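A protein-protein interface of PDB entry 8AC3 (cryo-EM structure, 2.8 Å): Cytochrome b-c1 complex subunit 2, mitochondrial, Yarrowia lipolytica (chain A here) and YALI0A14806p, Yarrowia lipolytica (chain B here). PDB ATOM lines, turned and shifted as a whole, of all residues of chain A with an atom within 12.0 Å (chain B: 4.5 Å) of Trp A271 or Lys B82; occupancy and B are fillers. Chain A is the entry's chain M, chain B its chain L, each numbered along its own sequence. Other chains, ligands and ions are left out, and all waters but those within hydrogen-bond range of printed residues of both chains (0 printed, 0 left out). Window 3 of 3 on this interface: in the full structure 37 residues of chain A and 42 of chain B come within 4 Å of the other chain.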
ATOM      1  N   GLY A 265     -23.749  24.448 -28.297  1.00  0.00           N
ATOM      2  CA  GLY A 265     -22.649  24.113 -29.185  1.00  0.00           C
ATOM      3  C   GLY A 265     -21.725  23.042 -28.609  1.00  0.00           C
ATOM      4  O   GLY A 265     -21.490  22.032 -29.277  1.00  0.00           O
ATOM      5  N   PRO A 266     -21.131  23.240 -27.398  1.00  0.00           N
ATOM      6  CA  PRO A 266     -20.292  22.210 -26.781  1.00  0.00           C
ATOM      7  C   PRO A 266     -21.142  21.068 -26.224  1.00  0.00           C
ATOM      8  O   PRO A 266     -22.324  21.257 -25.931  1.00  0.00           O
ATOM      9  CB  PRO A 266     -19.518  22.957 -25.680  1.00  0.00           C
ATOM     10  CG  PRO A 266     -20.402  24.138 -25.322  1.00  0.00           C
ATOM     11  CD  PRO A 266     -21.196  24.463 -26.572  1.00  0.00           C
ATOM     12  N   ALA A 267     -20.529  19.881 -26.115  1.00  0.00           N
ATOM     13  CA  ALA A 267     -21.208  18.682 -25.638  1.00  0.00           C
ATOM     14  C   ALA A 267     -21.164  18.614 -24.110  1.00  0.00           C
ATOM     15  O   ALA A 267     -20.207  19.071 -23.484  1.00  0.00           O
ATOM     16  CB  ALA A 267     -20.621  17.450 -26.290  1.00  0.00           C
ATOM     17  N   SER A 268     -22.217  18.040 -23.525  1.00  0.00           N
ATOM     18  CA  SER A 268     -22.372  18.025 -22.082  1.00  0.00           C
ATOM     19  C   SER A 268     -22.079  16.630 -21.540  1.00  0.00           C
ATOM     20  O   SER A 268     -22.467  16.313 -20.416  1.00  0.00           O
ATOM     21  CB  SER A 268     -23.732  18.533 -21.670  1.00  0.00           C
ATOM     22  OG  SER A 268     -24.772  17.872 -22.379  1.00  0.00           O
ATOM     23  N   MET A 269     -21.371  15.839 -22.355  1.00  0.00           N
ATOM     24  CA  MET A 269     -20.934  14.506 -21.998  1.00  0.00           C
ATOM     25  C   MET A 269     -19.872  14.035 -22.998  1.00  0.00           C
ATOM     26  O   MET A 269     -19.823  14.495 -24.138  1.00  0.00           O
ATOM     27  CB  MET A 269     -22.110  13.530 -21.865  1.00  0.00           C
ATOM     28  CG  MET A 269     -22.653  13.056 -23.154  1.00  0.00           C
ATOM     29  SD  MET A 269     -24.122  12.117 -22.771  1.00  0.00           S
ATOM     30  CE  MET A 269     -24.220  11.093 -24.234  1.00  0.00           C
ATOM     31  N   PRO A 270     -18.944  13.143 -22.592  1.00  0.00           N
ATOM     32  CA  PRO A 270     -17.779  12.819 -23.414  1.00  0.00           C
ATOM     33  C   PRO A 270     -18.170  12.037 -24.661  1.00  0.00           C
ATOM     34  O   PRO A 270     -19.151  11.299 -24.657  1.00  0.00           O
ATOM     35  CB  PRO A 270     -16.937  11.928 -22.493  1.00  0.00           C
ATOM     36  CG  PRO A 270     -17.477  12.192 -21.111  1.00  0.00           C
ATOM     37  CD  PRO A 270     -18.957  12.395 -21.328  1.00  0.00           C
ATOM     38  N   TRP A 271     -17.398  12.237 -25.736  1.00  0.00           N
ATOM     39  CA  TRP A 271     -17.519  11.468 -26.971  1.00  0.00           C
ATOM     40  C   TRP A 271     -18.919  11.598 -27.571  1.00  0.00           C
ATOM     41  O   TRP A 271     -19.386  10.695 -28.264  1.00  0.00           O
ATOM     42  CB  TRP A 271     -17.173   9.989 -26.745  1.00  0.00           C
ATOM     43  CG  TRP A 271     -16.092   9.753 -25.741  1.00  0.00           C
ATOM     44  CD1 TRP A 271     -16.212   9.148 -24.522  1.00  0.00           C
ATOM     45  CD2 TRP A 271     -14.713  10.135 -25.867  1.00  0.00           C
ATOM     46  NE1 TRP A 271     -14.997   9.104 -23.892  1.00  0.00           N
ATOM     47  CE2 TRP A 271     -14.061   9.713 -24.687  1.00  0.00           C
ATOM     48  CE3 TRP A 271     -13.973  10.792 -26.858  1.00  0.00           C
ATOM     49  CZ2 TRP A 271     -12.698   9.927 -24.476  1.00  0.00           C
ATOM     50  CZ3 TRP A 271     -12.627  11.001 -26.648  1.00  0.00           C
ATOM     51  CH2 TRP A 271     -12.001  10.577 -25.471  1.00  0.00           C
ATOM     52  N   SER A 272     -19.600  12.709 -27.286  1.00  0.00           N
ATOM     53  CA  SER A 272     -20.933  12.901 -27.826  1.00  0.00           C
ATOM     54  C   SER A 272     -20.962  14.174 -28.667  1.00  0.00           C
ATOM     55  O   SER A 272     -19.994  14.932 -28.675  1.00  0.00           O
ATOM     56  CB  SER A 272     -21.955  12.890 -26.724  1.00  0.00           C
ATOM     57  OG  SER A 272     -22.380  14.202 -26.402  1.00  0.00           O
ATOM     58  N   VAL A 273     -22.077  14.389 -29.369  1.00  0.00           N
ATOM     59  CA  VAL A 273     -22.225  15.583 -30.182  1.00  0.00           C
ATOM     60  C   VAL A 273     -22.954  16.654 -29.377  1.00  0.00           C
ATOM     61  O   VAL A 273     -22.493  17.790 -29.302  1.00  0.00           O
ATOM     62  CB  VAL A 273     -22.848  15.269 -31.558  1.00  0.00           C
ATOM     63  CG1 VAL A 273     -23.902  16.280 -31.989  1.00  0.00           C
ATOM     64  CG2 VAL A 273     -21.770  15.117 -32.615  1.00  0.00           C
ATOM     65  N   GLY A 274     -24.081  16.275 -28.763  1.00  0.00           N
ATOM     66  CA  GLY A 274     -24.874  17.187 -27.958  1.00  0.00           C
ATOM     67  C   GLY A 274     -26.246  17.392 -28.584  1.00  0.00           C
ATOM     68  O   GLY A 274     -26.439  17.104 -29.765  1.00  0.00           O
ATOM     69  N   ALA A 275     -27.189  17.901 -27.791  1.00  0.00           N
ATOM     70  CA  ALA A 275     -28.579  17.954 -28.212  1.00  0.00           C
ATOM     71  C   ALA A 275     -28.981  19.388 -28.558  1.00  0.00           C
ATOM     72  O   ALA A 275     -30.128  19.647 -28.929  1.00  0.00           O
ATOM     73  CB  ALA A 275     -29.448  17.342 -27.140  1.00  0.00           C
ATOM     74  N   ALA A 279     -24.959  22.171 -31.913  1.00  0.00           N
ATOM     75  CA  ALA A 279     -24.151  20.972 -31.774  1.00  0.00           C
ATOM     76  C   ALA A 279     -24.527  19.994 -32.882  1.00  0.00           C
ATOM     77  O   ALA A 279     -23.658  19.352 -33.469  1.00  0.00           O
ATOM     78  CB  ALA A 279     -24.328  20.381 -30.395  1.00  0.00           C
ATOM     79  N   GLN A 280     -25.833  19.964 -33.193  1.00  0.00           N
ATOM     80  CA  GLN A 280     -26.425  19.078 -34.187  1.00  0.00           C
ATOM     81  C   GLN A 280     -26.070  19.542 -35.601  1.00  0.00           C
ATOM     82  O   GLN A 280     -26.305  18.833 -36.576  1.00  0.00           O
ATOM     83  CB  GLN A 280     -27.943  18.992 -33.975  1.00  0.00           C
ATOM     84  CG  GLN A 280     -28.360  18.043 -32.852  1.00  0.00           C
ATOM     85  CD  GLN A 280     -28.063  16.588 -33.138  1.00  0.00           C
ATOM     86  OE1 GLN A 280     -28.179  16.118 -34.269  1.00  0.00           O
ATOM     87  NE2 GLN A 280     -27.673  15.856 -32.105  1.00  0.00           N
ATOM     88  N   THR A 282     -23.036  20.131 -36.431  1.00  0.00           N
ATOM     89  CA  THR A 282     -21.665  19.717 -36.685  1.00  0.00           C
ATOM     90  C   THR A 282     -21.591  18.251 -37.091  1.00  0.00           C
ATOM     91  O   THR A 282     -20.488  17.759 -37.308  1.00  0.00           O
ATOM     92  CB  THR A 282     -20.767  19.902 -35.458  1.00  0.00           C
ATOM     93  OG1 THR A 282     -21.269  19.082 -34.405  1.00  0.00           O
ATOM     94  CG2 THR A 282     -20.715  21.334 -34.991  1.00  0.00           C
ATOM     95  N   VAL A 283     -22.740  17.574 -37.225  1.00  0.00           N
ATOM     96  CA  VAL A 283     -22.725  16.119 -37.332  1.00  0.00           C
ATOM     97  C   VAL A 283     -22.091  15.672 -38.652  1.00  0.00           C
ATOM     98  O   VAL A 283     -22.484  16.118 -39.729  1.00  0.00           O
ATOM     99  CB  VAL A 283     -24.096  15.459 -37.067  1.00  0.00           C
ATOM    100  CG1 VAL A 283     -24.527  15.618 -35.617  1.00  0.00           C
ATOM    101  CG2 VAL A 283     -25.192  15.933 -38.014  1.00  0.00           C
ATOM    102  N   GLY A 284     -21.073  14.813 -38.526  1.00  0.00           N
ATOM    103  CA  GLY A 284     -20.331  14.289 -39.663  1.00  0.00           C
ATOM    104  C   GLY A 284     -19.100  15.129 -39.991  1.00  0.00           C
ATOM    105  O   GLY A 284     -18.428  14.892 -40.997  1.00  0.00           O
ATOM    106  N   THR A 285     -18.829  16.117 -39.134  1.00  0.00           N
ATOM    107  CA  THR A 285     -17.673  16.985 -39.280  1.00  0.00           C
ATOM    108  C   THR A 285     -16.883  17.004 -37.974  1.00  0.00           C
ATOM    109  O   THR A 285     -17.461  16.893 -36.891  1.00  0.00           O
ATOM    110  CB  THR A 285     -18.077  18.409 -39.688  1.00  0.00           C
ATOM    111  OG1 THR A 285     -18.982  18.901 -38.706  1.00  0.00           O
ATOM    112  CG2 THR A 285     -18.750  18.497 -41.040  1.00  0.00           C
ATOM    113  N   HIS A 286     -15.557  17.137 -38.104  1.00  0.00           N
ATOM    114  CA  HIS A 286     -14.683  17.363 -36.966  1.00  0.00           C
ATOM    115  C   HIS A 286     -14.550  18.867 -36.766  1.00  0.00           C
ATOM    116  O   HIS A 286     -13.487  19.448 -36.971  1.00  0.00           O
ATOM    117  CB  HIS A 286     -13.349  16.620 -37.138  1.00  0.00           C
ATOM    118  CG  HIS A 286     -13.515  15.194 -37.546  1.00  0.00           C
ATOM    119  ND1 HIS A 286     -14.212  14.279 -36.776  1.00  0.00           N
ATOM    120  CD2 HIS A 286     -13.099  14.526 -38.644  1.00  0.00           C
ATOM    121  CE1 HIS A 286     -14.210  13.107 -37.379  1.00  0.00           C
ATOM    122  NE2 HIS A 286     -13.533  13.232 -38.527  1.00  0.00           N
ATOM    123  N   THR A 287     -15.681  19.483 -36.429  1.00  0.00           N
ATOM    124  CA  THR A 287     -15.753  20.903 -36.155  1.00  0.00           C
ATOM    125  C   THR A 287     -16.429  21.079 -34.806  1.00  0.00           C
ATOM    126  O   THR A 287     -17.272  20.271 -34.416  1.00  0.00           O
ATOM    127  CB  THR A 287     -16.565  21.649 -37.222  1.00  0.00           C
ATOM    128  OG1 THR A 287     -17.843  21.015 -37.315  1.00  0.00           O
ATOM    129  CG2 THR A 287     -15.884  21.706 -38.572  1.00  0.00           C
ATOM    130  N   SER A 288     -16.029  22.138 -34.107  1.00  0.00           N
ATOM    131  CA  SER A 288     -16.728  22.532 -32.902  1.00  0.00           C
ATOM    132  C   SER A 288     -17.314  23.924 -33.081  1.00  0.00           C
ATOM    133  O   SER A 288     -16.876  24.700 -33.928  1.00  0.00           O
ATOM    134  CB  SER A 288     -15.850  22.428 -31.689  1.00  0.00           C
ATOM    135  OG  SER A 288     -14.566  22.947 -31.970  1.00  0.00           O
ATOM    136  N   HIS B  74     -10.743   1.878 -21.606  1.00  0.00           N
ATOM    137  CA  HIS B  74     -10.954   3.122 -22.318  1.00  0.00           C
ATOM    138  C   HIS B  74     -12.123   2.976 -23.284  1.00  0.00           C
ATOM    139  O   HIS B  74     -12.845   3.938 -23.542  1.00  0.00           O
ATOM    140  CB  HIS B  74      -9.670   3.561 -23.026  1.00  0.00           C
ATOM    141  CG  HIS B  74      -9.846   4.760 -23.896  1.00  0.00           C
ATOM    142  ND1 HIS B  74      -9.948   6.043 -23.392  1.00  0.00           N
ATOM    143  CD2 HIS B  74      -9.990   4.868 -25.235  1.00  0.00           C
ATOM    144  CE1 HIS B  74     -10.157   6.888 -24.378  1.00  0.00           C
ATOM    145  NE2 HIS B  74     -10.178   6.193 -25.522  1.00  0.00           N
ATOM    146  N   GLU B  77     -15.444   3.513 -21.459  1.00  0.00           N
ATOM    147  CA  GLU B  77     -15.676   4.932 -21.251  1.00  0.00           C
ATOM    148  C   GLU B  77     -16.434   5.550 -22.433  1.00  0.00           C
ATOM    149  O   GLU B  77     -17.233   6.462 -22.229  1.00  0.00           O
ATOM    150  CB  GLU B  77     -14.326   5.601 -20.991  1.00  0.00           C
ATOM    151  CG  GLU B  77     -14.428   7.074 -20.644  1.00  0.00           C
ATOM    152  CD  GLU B  77     -13.143   7.883 -20.717  1.00  0.00           C
ATOM    153  OE1 GLU B  77     -12.058   7.289 -20.576  1.00  0.00           O
ATOM    154  OE2 GLU B  77     -13.235   9.122 -20.897  1.00  0.00           O
ATOM    155  N   HIS B  78     -16.133   5.111 -23.664  1.00  0.00           N
ATOM    156  CA  HIS B  78     -16.782   5.639 -24.852  1.00  0.00           C
ATOM    157  C   HIS B  78     -18.183   5.093 -25.038  1.00  0.00           C
ATOM    158  O   HIS B  78     -18.902   5.631 -25.877  1.00  0.00           O
ATOM    159  CB  HIS B  78     -16.046   5.228 -26.127  1.00  0.00           C
ATOM    160  CG  HIS B  78     -14.852   6.066 -26.427  1.00  0.00           C
ATOM    161  ND1 HIS B  78     -14.755   6.850 -27.562  1.00  0.00           N
ATOM    162  CD2 HIS B  78     -13.682   6.213 -25.767  1.00  0.00           C
ATOM    163  CE1 HIS B  78     -13.579   7.448 -27.584  1.00  0.00           C
ATOM    164  NE2 HIS B  78     -12.904   7.082 -26.489  1.00  0.00           N
ATOM    165  N   LEU B  79     -18.462   3.934 -24.449  1.00  0.00           N
ATOM    166  CA  LEU B  79     -19.725   3.253 -24.668  1.00  0.00           C
ATOM    167  C   LEU B  79     -20.688   3.483 -23.516  1.00  0.00           C
ATOM    168  O   LEU B  79     -21.883   3.222 -23.652  1.00  0.00           O
ATOM    169  CB  LEU B  79     -19.460   1.756 -24.782  1.00  0.00           C
ATOM    170  CG  LEU B  79     -18.906   1.324 -26.121  1.00  0.00           C
ATOM    171  CD1 LEU B  79     -18.372  -0.083 -25.978  1.00  0.00           C
ATOM    172  CD2 LEU B  79     -19.986   1.381 -27.192  1.00  0.00           C
ATOM    173  N   ALA B  80     -20.159   3.921 -22.370  1.00  0.00           N
ATOM    174  CA  ALA B  80     -20.978   4.243 -21.218  1.00  0.00           C
ATOM    175  C   ALA B  80     -21.977   5.342 -21.575  1.00  0.00           C
ATOM    176  O   ALA B  80     -23.061   5.403 -21.004  1.00  0.00           O
ATOM    177  CB  ALA B  80     -20.098   4.643 -20.071  1.00  0.00           C
ATOM    178  N   PHE B  81     -21.627   6.162 -22.565  1.00  0.00           N
ATOM    179  CA  PHE B  81     -22.463   7.288 -22.921  1.00  0.00           C
ATOM    180  C   PHE B  81     -23.254   7.016 -24.193  1.00  0.00           C
ATOM    181  O   PHE B  81     -23.883   7.921 -24.731  1.00  0.00           O
ATOM    182  CB  PHE B  81     -21.609   8.549 -23.013  1.00  0.00           C
ATOM    183  CG  PHE B  81     -20.918   8.871 -21.716  1.00  0.00           C
ATOM    184  CD1 PHE B  81     -21.625   9.444 -20.669  1.00  0.00           C
ATOM    185  CD2 PHE B  81     -19.573   8.576 -21.531  1.00  0.00           C
ATOM    186  CE1 PHE B  81     -21.000   9.738 -19.467  1.00  0.00           C
ATOM    187  CE2 PHE B  81     -18.946   8.872 -20.329  1.00  0.00           C
ATOM    188  CZ  PHE B  81     -19.661   9.455 -19.302  1.00  0.00           C
ATOM    189  N   LYS B  82     -23.264   5.753 -24.623  1.00  0.00           N
ATOM    190  CA  LYS B  82     -23.870   5.417 -25.898  1.00  0.00           C
ATOM    191  C   LYS B  82     -25.207   4.715 -25.675  1.00  0.00           C
ATOM    192  O   LYS B  82     -25.754   4.120 -26.601  1.00  0.00           O
ATOM    193  CB  LYS B  82     -22.949   4.538 -26.752  1.00  0.00           C
ATOM    194  CG  LYS B  82     -21.679   5.164 -27.307  1.00  0.00           C
ATOM    195  CD  LYS B  82     -21.794   6.141 -28.459  1.00  0.00           C
ATOM    196  CE  LYS B  82     -20.810   7.280 -28.297  1.00  0.00           C
ATOM    197  NZ  LYS B  82     -21.387   8.485 -27.660  1.00  0.00           N
ATOM    198  N   GLY B  83     -25.741   4.797 -24.449  1.00  0.00           N
ATOM    199  CA  GLY B  83     -27.109   4.381 -24.190  1.00  0.00           C
ATOM    200  C   GLY B  83     -27.213   3.167 -23.270  1.00  0.00           C
ATOM    201  O   GLY B  83     -26.351   2.283 -23.259  1.00  0.00           O
ATOM    202  N   GLN B  89     -29.213   6.551 -26.768  1.00  0.00           N
ATOM    203  CA  GLN B  89     -28.129   7.523 -26.804  1.00  0.00           C
ATOM    204  C   GLN B  89     -28.703   8.938 -26.815  1.00  0.00           C
ATOM    205  O   GLN B  89     -28.167   9.838 -26.173  1.00  0.00           O
ATOM    206  CB  GLN B  89     -27.189   7.347 -27.996  1.00  0.00           C
ATOM    207  CG  GLN B  89     -26.039   8.336 -27.888  1.00  0.00           C
ATOM    208  CD  GLN B  89     -25.114   8.456 -29.072  1.00  0.00           C
ATOM    209  OE1 GLN B  89     -25.160   7.674 -30.019  1.00  0.00           O
ATOM    210  NE2 GLN B  89     -24.223   9.432 -28.993  1.00  0.00           N
ATOM    211  N   GLU B 147     -17.710   2.816 -32.528  1.00  0.00           N
ATOM    212  CA  GLU B 147     -16.703   3.468 -31.697  1.00  0.00           C
ATOM    213  C   GLU B 147     -15.317   2.971 -32.069  1.00  0.00           C
ATOM    214  O   GLU B 147     -14.315   3.643 -31.829  1.00  0.00           O
ATOM    215  CB  GLU B 147     -16.881   3.156 -30.208  1.00  0.00           C
ATOM    216  CG  GLU B 147     -17.862   4.064 -29.481  1.00  0.00           C
ATOM    217  CD  GLU B 147     -17.900   5.548 -29.834  1.00  0.00           C
ATOM    218  OE1 GLU B 147     -17.084   6.323 -29.288  1.00  0.00           O
ATOM    219  OE2 GLU B 147     -18.763   5.931 -30.658  1.00  0.00           O
ATOM    220  N   GLU B 154      -8.237   8.036 -32.749  1.00  0.00           N
ATOM    221  CA  GLU B 154      -7.645   8.684 -31.588  1.00  0.00           C
ATOM    222  C   GLU B 154      -6.184   8.273 -31.454  1.00  0.00           C
ATOM    223  O   GLU B 154      -5.395   9.037 -30.910  1.00  0.00           O
ATOM    224  CB  GLU B 154      -8.339   8.253 -30.303  1.00  0.00           C
ATOM    225  CG  GLU B 154      -9.471   9.137 -29.825  1.00  0.00           C
ATOM    226  CD  GLU B 154     -10.037   8.634 -28.504  1.00  0.00           C
ATOM    227  OE1 GLU B 154     -10.438   7.443 -28.438  1.00  0.00           O
ATOM    228  OE2 GLU B 154     -10.053   9.417 -27.532  1.00  0.00           O
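OE2 of Glu B77 is in hydrogen-bond range of NE1 of Trp A271, 3.5 Å away. The backbone carbonyl oxygen of Trp A271 lies within hydrogen-bond range of the side-chain amino group of Lys B82.
The side-chain carboxylate of Glu B154 is in hydrogen-bond range of a ring nitrogen (NE2) of His B78 (3.2 Å). A ring nitrogen (NE2) of His B78 sits at hydrogen-bond distance from a ring nitrogen (NE2) of His B74 (3.0 Å). OE1 of Glu B147 is in hydrogen-bond range of ND1 of His B78 (2.9 Å). The side-chain hydroxyl of Ser A272 sits at hydrogen-bond distance from the backbone carbonyl oxygen of Met A269 (3.4 Å). The side-chain amide nitrogen of Gln B89 sits close to the side-chain amino group of Lys B82. OE1 of Glu B154 is in hydrogen-bond range of NE2 of His B74 (3.2 Å).
Met A269 touches Phe B81. CD of Pro A270 touches CZ of Phe B81 (3.6 Å). Trp A271 touches His B74. CE1 of His B78 touches CD2 of Trp A271 (3.4 Å). Glu B154 touches Trp A271 (OE2 to CH2, 3.1 Å).
Of chain B, only His B74 (3.96 Å), Glu B77 (3.5 Å), His B78 (3.4 Å), Lys B82 (3.0 Å) and Glu B154 (3.1 Å) come within 4 Å of Trp A271. Lys B82 touches one residue of chain A. Glu B77 touches one residue of chain A. His B78 touches just one residue of chain A: Trp A271 (3.4 Å). No residue of chain A comes within 4 Å of Leu B79. No residue of chain A comes within 4 Å of Ala B80. Phe B81 touches just these residues of chain A: Met A269 and Pro A270. No residue of chain A comes within 4 Å of Gly B83. Of the printed residues of chain B, Pro A270 touches Phe B81. Printed residues of chain A within 4 Å of His B74: Trp A271. Of the printed residues of chain A, Glu B154 touches Trp A271. Of the printed residues of chain B, Met A269 touches Phe B81 (3.2 Å). His A286 touches none of the printed residues of chain B. The nearest printed residue of chain A that does not touch Glu B154 is Pro A270 (8.9 Å).
Hydrophobic or aromatic side chains of chain B that line the printed part of chain A: His B74, His B78 and Phe B81. Along chain B the printed residues that touch a printed residue of chain A span positions 74 to 154. Of the 20 printed residues of chain A, 3 touch a printed residue of chain B. Printed residues of chain A that touch a printed residue of chain B: Met A269, Pro A270 and Trp A271. Hydrophobic or aromatic side chains of chain A that line the printed part of chain B: Met A269, Pro A270 and Trp A271. Among the printed residues, no Asp or Glu carboxylate lies within 4 Å of a Lys or Arg side-chain nitrogen of the other chain.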
